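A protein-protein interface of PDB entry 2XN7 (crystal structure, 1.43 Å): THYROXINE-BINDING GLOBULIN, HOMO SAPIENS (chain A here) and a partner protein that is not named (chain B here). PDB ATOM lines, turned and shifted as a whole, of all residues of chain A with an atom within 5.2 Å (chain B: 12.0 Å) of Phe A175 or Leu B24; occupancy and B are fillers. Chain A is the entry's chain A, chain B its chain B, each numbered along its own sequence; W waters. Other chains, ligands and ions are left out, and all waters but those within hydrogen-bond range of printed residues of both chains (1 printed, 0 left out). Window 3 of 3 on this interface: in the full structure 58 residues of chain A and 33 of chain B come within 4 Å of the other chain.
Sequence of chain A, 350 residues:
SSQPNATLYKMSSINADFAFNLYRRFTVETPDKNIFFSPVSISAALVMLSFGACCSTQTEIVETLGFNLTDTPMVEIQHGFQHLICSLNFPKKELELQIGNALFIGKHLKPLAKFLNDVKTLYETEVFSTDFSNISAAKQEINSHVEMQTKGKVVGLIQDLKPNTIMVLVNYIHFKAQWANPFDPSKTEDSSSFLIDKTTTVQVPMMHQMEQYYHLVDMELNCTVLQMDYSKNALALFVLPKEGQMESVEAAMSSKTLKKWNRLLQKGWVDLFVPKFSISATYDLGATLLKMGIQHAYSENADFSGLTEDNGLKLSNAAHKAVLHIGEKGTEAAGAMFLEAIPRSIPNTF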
ATOM      1  N   PHE A  37       1.130  12.140  -0.037  1.00  0.00           N
ATOM      2  CA  PHE A  37       1.965  12.388   1.130  1.00  0.00           C
ATOM      3  C   PHE A  37       1.139  12.707   2.348  1.00  0.00           C
ATOM      4  O   PHE A  37      -0.054  12.996   2.243  1.00  0.00           O
ATOM      5  CB  PHE A  37       2.999  13.491   0.853  1.00  0.00           C
ATOM      6  CG  PHE A  37       2.431  14.880   0.663  1.00  0.00           C
ATOM      7  CD1 PHE A  37       1.869  15.270  -0.548  1.00  0.00           C
ATOM      8  CD2 PHE A  37       2.539  15.817   1.677  1.00  0.00           C
ATOM      9  CE1 PHE A  37       1.388  16.575  -0.716  1.00  0.00           C
ATOM     10  CE2 PHE A  37       2.072  17.103   1.515  1.00  0.00           C
ATOM     11  CZ  PHE A  37       1.505  17.489   0.320  1.00  0.00           C
ATOM     12  N   SER A  38       1.763  12.614   3.516  1.00  0.00           N
ATOM     13  CA  SER A  38       1.150  13.049   4.761  1.00  0.00           C
ATOM     14  C   SER A  38       1.722  14.385   5.188  1.00  0.00           C
ATOM     15  O   SER A  38       2.837  14.444   5.730  1.00  0.00           O
ATOM     16  CB  SER A  38       1.375  12.040   5.885  1.00  0.00           C
ATOM     17  OG  SER A  38       0.819  12.517   7.098  1.00  0.00           O
ATOM     18  N   PRO A  39       0.952  15.464   4.998  1.00  0.00           N
ATOM     19  CA  PRO A  39       1.456  16.766   5.434  1.00  0.00           C
ATOM     20  C   PRO A  39       1.665  16.820   6.951  1.00  0.00           C
ATOM     21  O   PRO A  39       2.635  17.415   7.410  1.00  0.00           O
ATOM     22  CB  PRO A  39       0.388  17.766   4.976  1.00  0.00           C
ATOM     23  CG  PRO A  39      -0.671  16.998   4.276  1.00  0.00           C
ATOM     24  CD  PRO A  39      -0.376  15.545   4.358  1.00  0.00           C
ATOM     25  N   VAL A  40       0.782  16.190   7.727  1.00  0.00           N
ATOM     26  CA  VAL A  40       0.933  16.224   9.190  1.00  0.00           C
ATOM     27  C   VAL A  40       2.225  15.523   9.617  1.00  0.00           C
ATOM     28  O   VAL A  40       2.901  15.975  10.543  1.00  0.00           O
ATOM     29  CB  VAL A  40      -0.300  15.669   9.936  1.00  0.00           C
ATOM     30  CG1 VAL A  40      -0.419  14.174   9.757  1.00  0.00           C
ATOM     31  CG2 VAL A  40      -0.223  16.047  11.417  1.00  0.00           C
ATOM     32  N   LEU A  88      -4.700  13.603  18.096  1.00  0.00           N
ATOM     33  CA  LEU A  88      -4.793  12.631  17.002  1.00  0.00           C
ATOM     34  C   LEU A  88      -4.674  11.195  17.510  1.00  0.00           C
ATOM     35  O   LEU A  88      -5.346  10.304  17.003  1.00  0.00           O
ATOM     36  CB  LEU A  88      -3.746  12.914  15.915  1.00  0.00           C
ATOM     37  CG  LEU A  88      -3.898  14.202  15.094  1.00  0.00           C
ATOM     38  CD1 LEU A  88      -2.684  14.380  14.206  1.00  0.00           C
ATOM     39  CD2 LEU A  88      -5.178  14.231  14.238  1.00  0.00           C
ATOM     40  N   LEU A  95     -11.724   3.639  14.544  1.00  0.00           N
ATOM     41  CA  LEU A  95     -10.663   4.330  13.803  1.00  0.00           C
ATOM     42  C   LEU A  95      -9.289   3.940  14.333  1.00  0.00           C
ATOM     43  O   LEU A  95      -9.006   4.118  15.512  1.00  0.00           O
ATOM     44  CB  LEU A  95     -10.829   5.849  13.917  1.00  0.00           C
ATOM     45  CG  LEU A  95      -9.732   6.731  13.289  1.00  0.00           C
ATOM     46  CD1 LEU A  95      -9.666   6.541  11.773  1.00  0.00           C
ATOM     47  CD2 LEU A  95      -9.924   8.205  13.644  1.00  0.00           C
ATOM     48  N   GLU A  96      -8.438   3.412  13.464  1.00  0.00           N
ATOM     49  CA  GLU A  96      -7.020   3.249  13.769  1.00  0.00           C
ATOM     50  C   GLU A  96      -6.282   4.490  13.270  1.00  0.00           C
ATOM     51  O   GLU A  96      -6.261   4.773  12.080  1.00  0.00           O
ATOM     52  CB  GLU A  96      -6.446   1.991  13.107  1.00  0.00           C
ATOM     53  CG  GLU A  96      -6.957   0.684  13.685  1.00  0.00           C
ATOM     54  CD  GLU A  96      -6.206  -0.539  13.185  1.00  0.00           C
ATOM     55  OE1 GLU A  96      -5.331  -0.416  12.309  1.00  0.00           O
ATOM     56  OE2 GLU A  96      -6.494  -1.649  13.680  1.00  0.00           O
ATOM     57  N   LEU A  97      -5.714   5.252  14.191  1.00  0.00           N
ATOM     58  CA  LEU A  97      -4.894   6.392  13.831  1.00  0.00           C
ATOM     59  C   LEU A  97      -3.816   6.574  14.884  1.00  0.00           C
ATOM     60  O   LEU A  97      -4.100   6.853  16.040  1.00  0.00           O
ATOM     61  CB  LEU A  97      -5.731   7.660  13.714  1.00  0.00           C
ATOM     62  CG  LEU A  97      -4.965   8.954  13.457  1.00  0.00           C
ATOM     63  CD1 LEU A  97      -4.134   8.884  12.174  1.00  0.00           C
ATOM     64  CD2 LEU A  97      -5.955  10.109  13.403  1.00  0.00           C
ATOM     65  N   ILE A 173       3.036   7.842  10.587  1.00  0.00           N
ATOM     66  CA  ILE A 173       1.590   7.909  10.727  1.00  0.00           C
ATOM     67  C   ILE A 173       0.972   6.657  10.093  1.00  0.00           C
ATOM     68  O   ILE A 173       1.390   6.220   9.020  1.00  0.00           O
ATOM     69  CB  ILE A 173       1.016   9.199  10.098  1.00  0.00           C
ATOM     70  CG1 ILE A 173      -0.508   9.249  10.272  1.00  0.00           C
ATOM     71  CG2 ILE A 173       1.404   9.327   8.640  1.00  0.00           C
ATOM     72  CD1 ILE A 173      -1.099  10.613   9.931  1.00  0.00           C
ATOM     73  N   HIS A 174       0.016   6.058  10.799  1.00  0.00           N
ATOM     74  CA  HIS A 174      -0.781   4.950  10.258  1.00  0.00           C
ATOM     75  C   HIS A 174      -2.259   5.241  10.470  1.00  0.00           C
ATOM     76  O   HIS A 174      -2.661   5.689  11.535  1.00  0.00           O
ATOM     77  CB  HIS A 174      -0.398   3.598  10.870  1.00  0.00           C
ATOM     78  CG  HIS A 174      -1.293   2.487  10.422  1.00  0.00           C
ATOM     79  ND1 HIS A 174      -2.348   2.047  11.184  1.00  0.00           N
ATOM     80  CD2 HIS A 174      -1.340   1.780   9.268  1.00  0.00           C
ATOM     81  CE1 HIS A 174      -2.998   1.099  10.529  1.00  0.00           C
ATOM     82  NE2 HIS A 174      -2.407   0.919   9.362  1.00  0.00           N
ATOM     83  N   PHE A 175      -3.063   4.985   9.434  1.00  0.00           N
ATOM     84  CA  PHE A 175      -4.482   5.288   9.419  1.00  0.00           C
ATOM     85  C   PHE A 175      -5.232   4.145   8.770  1.00  0.00           C
ATOM     86  O   PHE A 175      -4.897   3.726   7.670  1.00  0.00           O
ATOM     87  CB  PHE A 175      -4.709   6.549   8.593  1.00  0.00           C
ATOM     88  CG  PHE A 175      -6.162   6.880   8.311  1.00  0.00           C
ATOM     89  CD1 PHE A 175      -6.925   7.591   9.221  1.00  0.00           C
ATOM     90  CD2 PHE A 175      -6.754   6.538   7.100  1.00  0.00           C
ATOM     91  CE1 PHE A 175      -8.253   7.927   8.945  1.00  0.00           C
ATOM     92  CE2 PHE A 175      -8.090   6.872   6.840  1.00  0.00           C
ATOM     93  CZ  PHE A 175      -8.826   7.546   7.762  1.00  0.00           C
ATOM     94  N   LYS A 176      -6.230   3.610   9.469  1.00  0.00           N
ATOM     95  CA  LYS A 176      -7.092   2.606   8.867  1.00  0.00           C
ATOM     96  C   LYS A 176      -8.496   2.857   9.352  1.00  0.00           C
ATOM     97  O   LYS A 176      -8.762   2.929  10.556  1.00  0.00           O
ATOM     98  CB  LYS A 176      -6.630   1.184   9.193  1.00  0.00           C
ATOM     99  CG  LYS A 176      -7.419   0.136   8.447  1.00  0.00           C
ATOM    100  CD  LYS A 176      -6.979  -1.271   8.811  1.00  0.00           C
ATOM    101  CE  LYS A 176      -7.628  -2.259   7.879  1.00  0.00           C
ATOM    102  NZ  LYS A 176      -7.486  -3.649   8.359  1.00  0.00           N
ATOM    103  N   ALA A 177      -9.411   2.981   8.404  1.00  0.00           N
ATOM    104  CA  ALA A 177     -10.772   3.366   8.711  1.00  0.00           C
ATOM    105  C   ALA A 177     -11.729   2.680   7.760  1.00  0.00           C
ATOM    106  O   ALA A 177     -11.357   2.317   6.635  1.00  0.00           O
ATOM    107  CB  ALA A 177     -10.940   4.871   8.592  1.00  0.00           C
ATOM    108  N   TYR A 230     -15.833   8.328   6.861  1.00  0.00           N
ATOM    109  CA  TYR A 230     -15.464   7.098   7.525  1.00  0.00           C
ATOM    110  C   TYR A 230     -16.405   6.938   8.715  1.00  0.00           C
ATOM    111  O   TYR A 230     -17.212   7.800   9.000  1.00  0.00           O
ATOM    112  CB  TYR A 230     -13.982   7.096   7.914  1.00  0.00           C
ATOM    113  CG  TYR A 230     -13.082   7.143   6.686  1.00  0.00           C
ATOM    114  CD1 TYR A 230     -12.420   8.315   6.337  1.00  0.00           C
ATOM    115  CD2 TYR A 230     -12.941   6.043   5.843  1.00  0.00           C
ATOM    116  CE1 TYR A 230     -11.607   8.379   5.239  1.00  0.00           C
ATOM    117  CE2 TYR A 230     -12.118   6.103   4.705  1.00  0.00           C
ATOM    118  CZ  TYR A 230     -11.452   7.286   4.415  1.00  0.00           C
ATOM    119  OH  TYR A 230     -10.641   7.405   3.304  1.00  0.00           O
ATOM    120  N   ALA A 234     -13.418  10.884  10.871  1.00  0.00           N
ATOM    121  CA  ALA A 234     -12.578  11.123   9.696  1.00  0.00           C
ATOM    122  C   ALA A 234     -13.411  11.087   8.421  1.00  0.00           C
ATOM    123  O   ALA A 234     -14.508  10.534   8.400  1.00  0.00           O
ATOM    124  CB  ALA A 234     -11.474  10.101   9.634  1.00  0.00           C
ATOM    125  N   THR A 331     -10.342   2.558   3.848  1.00  0.00           N
ATOM    126  CA  THR A 331      -9.069   3.116   3.395  1.00  0.00           C
ATOM    127  C   THR A 331      -8.004   2.776   4.417  1.00  0.00           C
ATOM    128  O   THR A 331      -8.261   2.808   5.617  1.00  0.00           O
ATOM    129  CB  THR A 331      -9.168   4.658   3.228  1.00  0.00           C
ATOM    130  OG1 THR A 331     -10.144   4.983   2.230  1.00  0.00           O
ATOM    131  CG2 THR A 331      -7.828   5.318   2.857  1.00  0.00           C
ATOM    132  N   GLU A 332      -6.810   2.457   3.933  1.00  0.00           N
ATOM    133  CA  GLU A 332      -5.625   2.316   4.789  1.00  0.00           C
ATOM    134  C   GLU A 332      -4.515   3.160   4.159  1.00  0.00           C
ATOM    135  O   GLU A 332      -4.218   3.016   2.975  1.00  0.00           O
ATOM    136  CB  GLU A 332      -5.206   0.842   4.993  1.00  0.00           C
ATOM    137  CG  GLU A 332      -4.048   0.671   5.974  1.00  0.00           C
ATOM    138  CD  GLU A 332      -3.914  -0.743   6.529  1.00  0.00           C
ATOM    139  OE1 GLU A 332      -4.452  -1.682   5.906  1.00  0.00           O
ATOM    140  OE2 GLU A 332      -3.249  -0.921   7.570  1.00  0.00           O
ATOM    141  N   ALA A 333      -3.909   4.027   4.956  1.00  0.00           N
ATOM    142  CA  ALA A 333      -2.842   4.897   4.476  1.00  0.00           C
ATOM    143  C   ALA A 333      -1.774   4.995   5.560  1.00  0.00           C
ATOM    144  O   ALA A 333      -2.070   4.895   6.747  1.00  0.00           O
ATOM    145  CB  ALA A 333      -3.383   6.282   4.107  1.00  0.00           C
ATOM    146  N   ALA A 334      -0.536   5.175   5.142  1.00  0.00           N
ATOM    147  CA  ALA A 334       0.543   5.371   6.089  1.00  0.00           C
ATOM    148  C   ALA A 334       1.612   6.252   5.487  1.00  0.00           C
ATOM    149  O   ALA A 334       1.708   6.375   4.276  1.00  0.00           O
ATOM    150  CB  ALA A 334       1.107   4.018   6.527  1.00  0.00           C
ATOM    151  N   LEU B  13      -7.304  14.053  -3.723  1.00  0.00           N
ATOM    152  CA  LEU B  13      -7.838  13.364  -2.570  1.00  0.00           C
ATOM    153  C   LEU B  13      -7.271  13.978  -1.304  1.00  0.00           C
ATOM    154  O   LEU B  13      -6.062  14.184  -1.212  1.00  0.00           O
ATOM    155  CB  LEU B  13      -7.443  11.890  -2.617  1.00  0.00           C
ATOM    156  CG  LEU B  13      -7.786  11.009  -1.417  1.00  0.00           C
ATOM    157  CD1 LEU B  13      -9.312  10.851  -1.256  1.00  0.00           C
ATOM    158  CD2 LEU B  13      -7.131   9.619  -1.541  1.00  0.00           C
ATOM    159  N   LEU B  14      -8.135  14.240  -0.331  1.00  0.00           N
ATOM    160  CA  LEU B  14      -7.723  14.652   1.006  1.00  0.00           C
ATOM    161  C   LEU B  14      -8.319  13.652   2.007  1.00  0.00           C
ATOM    162  O   LEU B  14      -9.486  13.291   1.874  1.00  0.00           O
ATOM    163  CB  LEU B  14      -8.259  16.057   1.335  1.00  0.00           C
ATOM    164  CG  LEU B  14      -7.708  17.243   0.552  1.00  0.00           C
ATOM    165  CD1 LEU B  14      -8.330  17.363  -0.802  1.00  0.00           C
ATOM    166  CD2 LEU B  14      -7.931  18.495   1.376  1.00  0.00           C
ATOM    167  N   ILE B  15      -7.541  13.255   3.012  1.00  0.00           N
ATOM    168  CA  ILE B  15      -8.052  12.480   4.147  1.00  0.00           C
ATOM    169  C   ILE B  15      -7.929  13.397   5.354  1.00  0.00           C
ATOM    170  O   ILE B  15      -6.825  13.852   5.673  1.00  0.00           O
ATOM    171  CB  ILE B  15      -7.283  11.165   4.372  1.00  0.00           C
ATOM    172  CG1 ILE B  15      -7.437  10.277   3.134  1.00  0.00           C
ATOM    173  CG2 ILE B  15      -7.778  10.456   5.651  1.00  0.00           C
ATOM    174  CD1 ILE B  15      -6.601   9.052   3.155  1.00  0.00           C
ATOM    175  N   LEU B  16      -9.067  13.702   5.967  1.00  0.00           N
ATOM    176  CA  LEU B  16      -9.144  14.661   7.052  1.00  0.00           C
ATOM    177  C   LEU B  16      -9.595  14.020   8.346  1.00  0.00           C
ATOM    178  O   LEU B  16     -10.469  13.157   8.345  1.00  0.00           O
ATOM    179  CB  LEU B  16     -10.116  15.781   6.678  1.00  0.00           C
ATOM    180  CG  LEU B  16      -9.701  16.761   5.576  1.00  0.00           C
ATOM    181  CD1 LEU B  16     -10.895  17.151   4.703  1.00  0.00           C
ATOM    182  CD2 LEU B  16      -9.048  17.981   6.220  1.00  0.00           C
ATOM    183  N   GLU B  17      -8.986  14.440   9.453  1.00  0.00           N
ATOM    184  CA  GLU B  17      -9.459  14.091  10.784  1.00  0.00           C
ATOM    185  C   GLU B  17     -10.345  15.239  11.285  1.00  0.00           C
ATOM    186  O   GLU B  17      -9.981  16.410  11.185  1.00  0.00           O
ATOM    187  CB  GLU B  17      -8.275  13.835  11.734  1.00  0.00           C
ATOM    188  CG  GLU B  17      -8.634  13.177  13.075  1.00  0.00           C
ATOM    189  CD  GLU B  17      -9.082  14.166  14.151  1.00  0.00           C
ATOM    190  OE1 GLU B  17      -8.846  15.371  13.996  1.00  0.00           O
ATOM    191  OE2 GLU B  17      -9.678  13.732  15.150  1.00  0.00           O
ATOM    192  N   ARG B  18     -11.513  14.897  11.821  1.00  0.00           N
ATOM    193  CA  ARG B  18     -12.536  15.905  12.120  1.00  0.00           C
ATOM    194  C   ARG B  18     -12.262  16.779  13.341  1.00  0.00           C
ATOM    195  O   ARG B  18     -12.356  18.011  13.265  1.00  0.00           O
ATOM    196  CB  ARG B  18     -13.905  15.242  12.296  1.00  0.00           C
ATOM    197  CG  ARG B  18     -14.730  15.177  11.049  1.00  0.00           C
ATOM    198  CD  ARG B  18     -16.201  15.134  11.403  1.00  0.00           C
ATOM    199  NE  ARG B  18     -17.042  15.207  10.215  1.00  0.00           N
ATOM    200  CZ  ARG B  18     -17.283  14.194   9.386  1.00  0.00           C
ATOM    201  NH1 ARG B  18     -18.066  14.388   8.336  1.00  0.00           N
ATOM    202  NH2 ARG B  18     -16.746  12.994   9.590  1.00  0.00           N
ATOM    203  N   SER B  19     -11.929  16.148  14.462  1.00  0.00           N
ATOM    204  CA  SER B  19     -11.807  16.865  15.741  1.00  0.00           C
ATOM    205  C   SER B  19     -10.732  17.964  15.749  1.00  0.00           C
ATOM    206  O   SER B  19     -10.900  18.983  16.423  1.00  0.00           O
ATOM    207  CB  SER B  19     -11.567  15.886  16.895  1.00  0.00           C
ATOM    208  OG  SER B  19     -10.221  15.472  16.967  1.00  0.00           O
ATOM    209  N   THR B  20      -9.641  17.755  15.011  1.00  0.00           N
ATOM    210  CA  THR B  20      -8.552  18.731  14.909  1.00  0.00           C
ATOM    211  C   THR B  20      -8.556  19.486  13.577  1.00  0.00           C
ATOM    212  O   THR B  20      -7.785  20.424  13.403  1.00  0.00           O
ATOM    213  CB  THR B  20      -7.173  18.053  15.069  1.00  0.00           C
ATOM    214  OG1 THR B  20      -6.901  17.221  13.934  1.00  0.00           O
ATOM    215  CG2 THR B  20      -7.125  17.218  16.348  1.00  0.00           C
ATOM    216  N   ARG B  21      -9.407  19.056  12.647  1.00  0.00           N
ATOM    217  CA  ARG B  21      -9.466  19.589  11.287  1.00  0.00           C
ATOM    218  C   ARG B  21      -8.131  19.456  10.564  1.00  0.00           C
ATOM    219  O   ARG B  21      -7.711  20.366   9.852  1.00  0.00           O
ATOM    220  CB  ARG B  21      -9.972  21.043  11.290  1.00  0.00           C
ATOM    221  CG  ARG B  21     -11.332  21.179  11.934  1.00  0.00           C
ATOM    222  CD  ARG B  21     -11.913  22.582  11.838  1.00  0.00           C
ATOM    223  NE  ARG B  21     -13.237  22.632  12.461  1.00  0.00           N
ATOM    224  CZ  ARG B  21     -14.002  23.719  12.553  1.00  0.00           C
ATOM    225  NH1 ARG B  21     -13.586  24.889  12.071  1.00  0.00           N
ATOM    226  NH2 ARG B  21     -15.190  23.641  13.144  1.00  0.00           N
ATOM    227  N   SER B  22      -7.451  18.341  10.777  1.00  0.00           N
ATOM    228  CA  SER B  22      -6.132  18.119  10.196  1.00  0.00           C
ATOM    229  C   SER B  22      -6.209  17.356   8.885  1.00  0.00           C
ATOM    230  O   SER B  22      -6.917  16.357   8.783  1.00  0.00           O
ATOM    231  CB  SER B  22      -5.261  17.302  11.145  1.00  0.00           C
ATOM    232  OG  SER B  22      -4.937  18.029  12.304  1.00  0.00           O
ATOM    233  N   ILE B  23      -5.417  17.790   7.918  1.00  0.00           N
ATOM    234  CA  ILE B  23      -5.199  17.021   6.701  1.00  0.00           C
ATOM    235  C   ILE B  23      -4.138  15.971   7.011  1.00  0.00           C
ATOM    236  O   ILE B  23      -2.950  16.289   7.208  1.00  0.00           O
ATOM    237  CB  ILE B  23      -4.735  17.891   5.517  1.00  0.00           C
ATOM    238  CG1 ILE B  23      -5.761  19.003   5.186  1.00  0.00           C
ATOM    239  CG2 ILE B  23      -4.512  17.016   4.290  1.00  0.00           C
ATOM    240  CD1 ILE B  23      -5.292  19.942   4.099  1.00  0.00           C
ATOM    241  N   LEU B  24      -4.574  14.721   7.104  1.00  0.00           N
ATOM    242  CA  LEU B  24      -3.684  13.612   7.391  1.00  0.00           C
ATOM    243  C   LEU B  24      -2.916  13.183   6.158  1.00  0.00           C
ATOM    244  O   LEU B  24      -1.721  12.862   6.239  1.00  0.00           O
ATOM    245  CB  LEU B  24      -4.473  12.422   7.913  1.00  0.00           C
ATOM    246  CG  LEU B  24      -5.320  12.632   9.173  1.00  0.00           C
ATOM    247  CD1 LEU B  24      -6.026  11.347   9.566  1.00  0.00           C
ATOM    248  CD2 LEU B  24      -4.492  13.134  10.336  1.00  0.00           C
ATOM    249  N   PHE B  25      -3.614  13.146   5.023  1.00  0.00           N
ATOM    250  CA  PHE B  25      -3.022  12.781   3.739  1.00  0.00           C
ATOM    251  C   PHE B  25      -3.591  13.661   2.627  1.00  0.00           C
ATOM    252  O   PHE B  25      -4.753  14.061   2.685  1.00  0.00           O
ATOM    253  CB  PHE B  25      -3.318  11.315   3.425  1.00  0.00           C
ATOM    254  CG  PHE B  25      -2.747  10.352   4.439  1.00  0.00           C
ATOM    255  CD1 PHE B  25      -1.441   9.894   4.340  1.00  0.00           C
ATOM    256  CD2 PHE B  25      -3.517   9.920   5.501  1.00  0.00           C
ATOM    257  CE1 PHE B  25      -0.909   9.013   5.282  1.00  0.00           C
ATOM    258  CE2 PHE B  25      -2.992   9.049   6.449  1.00  0.00           C
ATOM    259  CZ  PHE B  25      -1.677   8.599   6.338  1.00  0.00           C
ATOM    260  N   LEU B  26      -2.785  13.908   1.596  1.00  0.00           N
ATOM    261  CA  LEU B  26      -3.149  14.735   0.465  1.00  0.00           C
ATOM    262  C   LEU B  26      -2.504  14.150  -0.770  1.00  0.00           C
ATOM    263  O   LEU B  26      -1.316  13.794  -0.761  1.00  0.00           O
ATOM    264  CB  LEU B  26      -2.619  16.162   0.650  1.00  0.00           C
ATOM    265  CG  LEU B  26      -2.807  17.202  -0.470  1.00  0.00           C
ATOM    266  CD1 LEU B  26      -4.258  17.385  -0.820  1.00  0.00           C
ATOM    267  CD2 LEU B  26      -2.198  18.565  -0.104  1.00  0.00           C
ATOM    268  N   GLY B  27      -3.270  14.065  -1.851  1.00  0.00           N
ATOM    269  CA  GLY B  27      -2.705  13.539  -3.062  1.00  0.00           C
ATOM    270  C   GLY B  27      -3.460  13.879  -4.315  1.00  0.00           C
ATOM    271  O   GLY B  27      -4.514  14.498  -4.285  1.00  0.00           O
ATOM    272  N   LYS B  28      -2.868  13.451  -5.416  1.00  0.00           N
ATOM    273  CA  LYS B  28      -3.492  13.485  -6.728  1.00  0.00           C
ATOM    274  C   LYS B  28      -3.257  12.133  -7.371  1.00  0.00           C
ATOM    275  O   LYS B  28      -2.126  11.655  -7.419  1.00  0.00           O
ATOM    276  CB  LYS B  28      -2.901  14.571  -7.602  1.00  0.00           C
ATOM    277  CG  LYS B  28      -3.414  14.523  -9.039  1.00  0.00           C
ATOM    278  CD  LYS B  28      -2.979  15.690  -9.876  1.00  0.00           C
ATOM    279  CE  LYS B  28      -1.464  15.809  -9.986  1.00  0.00           C
ATOM    280  NZ  LYS B  28      -1.028  16.948 -10.875  1.00  0.00           N
HETATM  281  O   HOH W   1     -16.729  10.463  10.439  1.00  0.00           O
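Phe A175 touches three residues of chain B.
Of chain A, only Ser A38, Pro A39, Val A40 and Phe A175 come within 4 Å of Leu B24.
Printed residues of chain B within 4 Å of Leu A88: Glu B17 and Thr B20.
No residue of chain B comes within 4 Å of Glu A96.
No residue of chain B comes within 4 Å of Lys A176.
Of chain B, only Ile B15 comes within 4 Å of Thr A331.
No residue of chain B comes within 4 Å of Glu A332.
Of chain B, only Phe B25 comes within 4 Å of Ala A333.
Ala A334 touches one residue of chain B.
Printed residues of chain A within 4 Å of Ile B23: Pro A39 (3.8 Å) and Val A40 (3.8 Å).
Of the printed residues of chain B, Pro A39 touches Ile B23 (3.8 Å), Leu B24 (3.5 Å) and Phe B25 (3.9 Å).
Of the printed residues of chain A, Arg B18 touches Ala A234.
Gly B27 touches none of the printed residues of chain A.
Hydrophobic or aromatic side chains of chain A that line the printed part of chain B: Phe A37, Pro A39, Val A40, Leu A88, Ile A173, Phe A175, Ala A234 and Ala A333.
Along chain A the printed residues that touch a printed residue of chain B span positions 37 to 334.
Of the 16 printed residues of chain B, 9 touch a printed residue of chain A.
Among the printed residues, 20 pairs touch across the chains.
Water W1 lies within hydrogen-bond range of NH2 of Arg B18 (2.7 Å), O of Ala A234 (3.0 Å) and O of Tyr A230 (3.1 Å).
The backbone NH (N) of Thr A331 is in hydrogen-bond range of the backbone carbonyl oxygen (O) of Ala A177 (3.0 Å).
OH of Tyr A230 is in hydrogen-bond range of OG1 of Thr A331 (2.7 Å).
The backbone NH (N) of Leu B24 lies within hydrogen-bond range of the backbone carbonyl oxygen (O) of Ile B15 (2.8 Å).
N of Ile B15 lies within hydrogen-bond range of O of Phe B25 (2.9 Å).
OG1 of Thr B20 lies within hydrogen-bond range of OE1 of Glu B17 (2.7 Å).
The backbone NH (N) of Glu B17 lies within hydrogen-bond range of the backbone carbonyl oxygen (O) of Ser B22.
Among the printed residues, merely in contact across the chains: Ala A234 with Leu B16 (3.2 Å), Phe A37 with Phe B25 (3.3 Å), Leu A88 with Thr B20 (3.5 Å), Ala A234 with Arg B18 (3.5 Å), Pro A39 with Leu B24 (3.5 Å), Ala A333 with Phe B25 (3.6 Å), Phe A175 with Phe B25 (3.7 Å), Ala A334 with Phe B25 (3.7 Å), Phe A175 with Ile B15 (3.7 Å), Val A40 with Ile B23 (3.8 Å), Pro A39 with Ile B23 (3.8 Å), Leu A88 with Glu B17 (3.8 Å), Ser A38 with Phe B25 (3.8 Å), Pro A39 with Phe B25 (3.9 Å), Phe A175 with Leu B24 (3.9 Å), Ile A173 with Phe B25 (3.9 Å), Thr A331 with Ile B15 (3.9 Å) and Val A40 with Leu B24 (3.97 Å).
The backbone NH of Leu B26 is in hydrogen-bond range of the backbone carbonyl oxygen of Phe A37.
The side-chain hydroxyl (OG) of Ser A38 is in hydrogen-bond range of the backbone carbonyl oxygen (O) of Leu B24 (2.7 Å).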
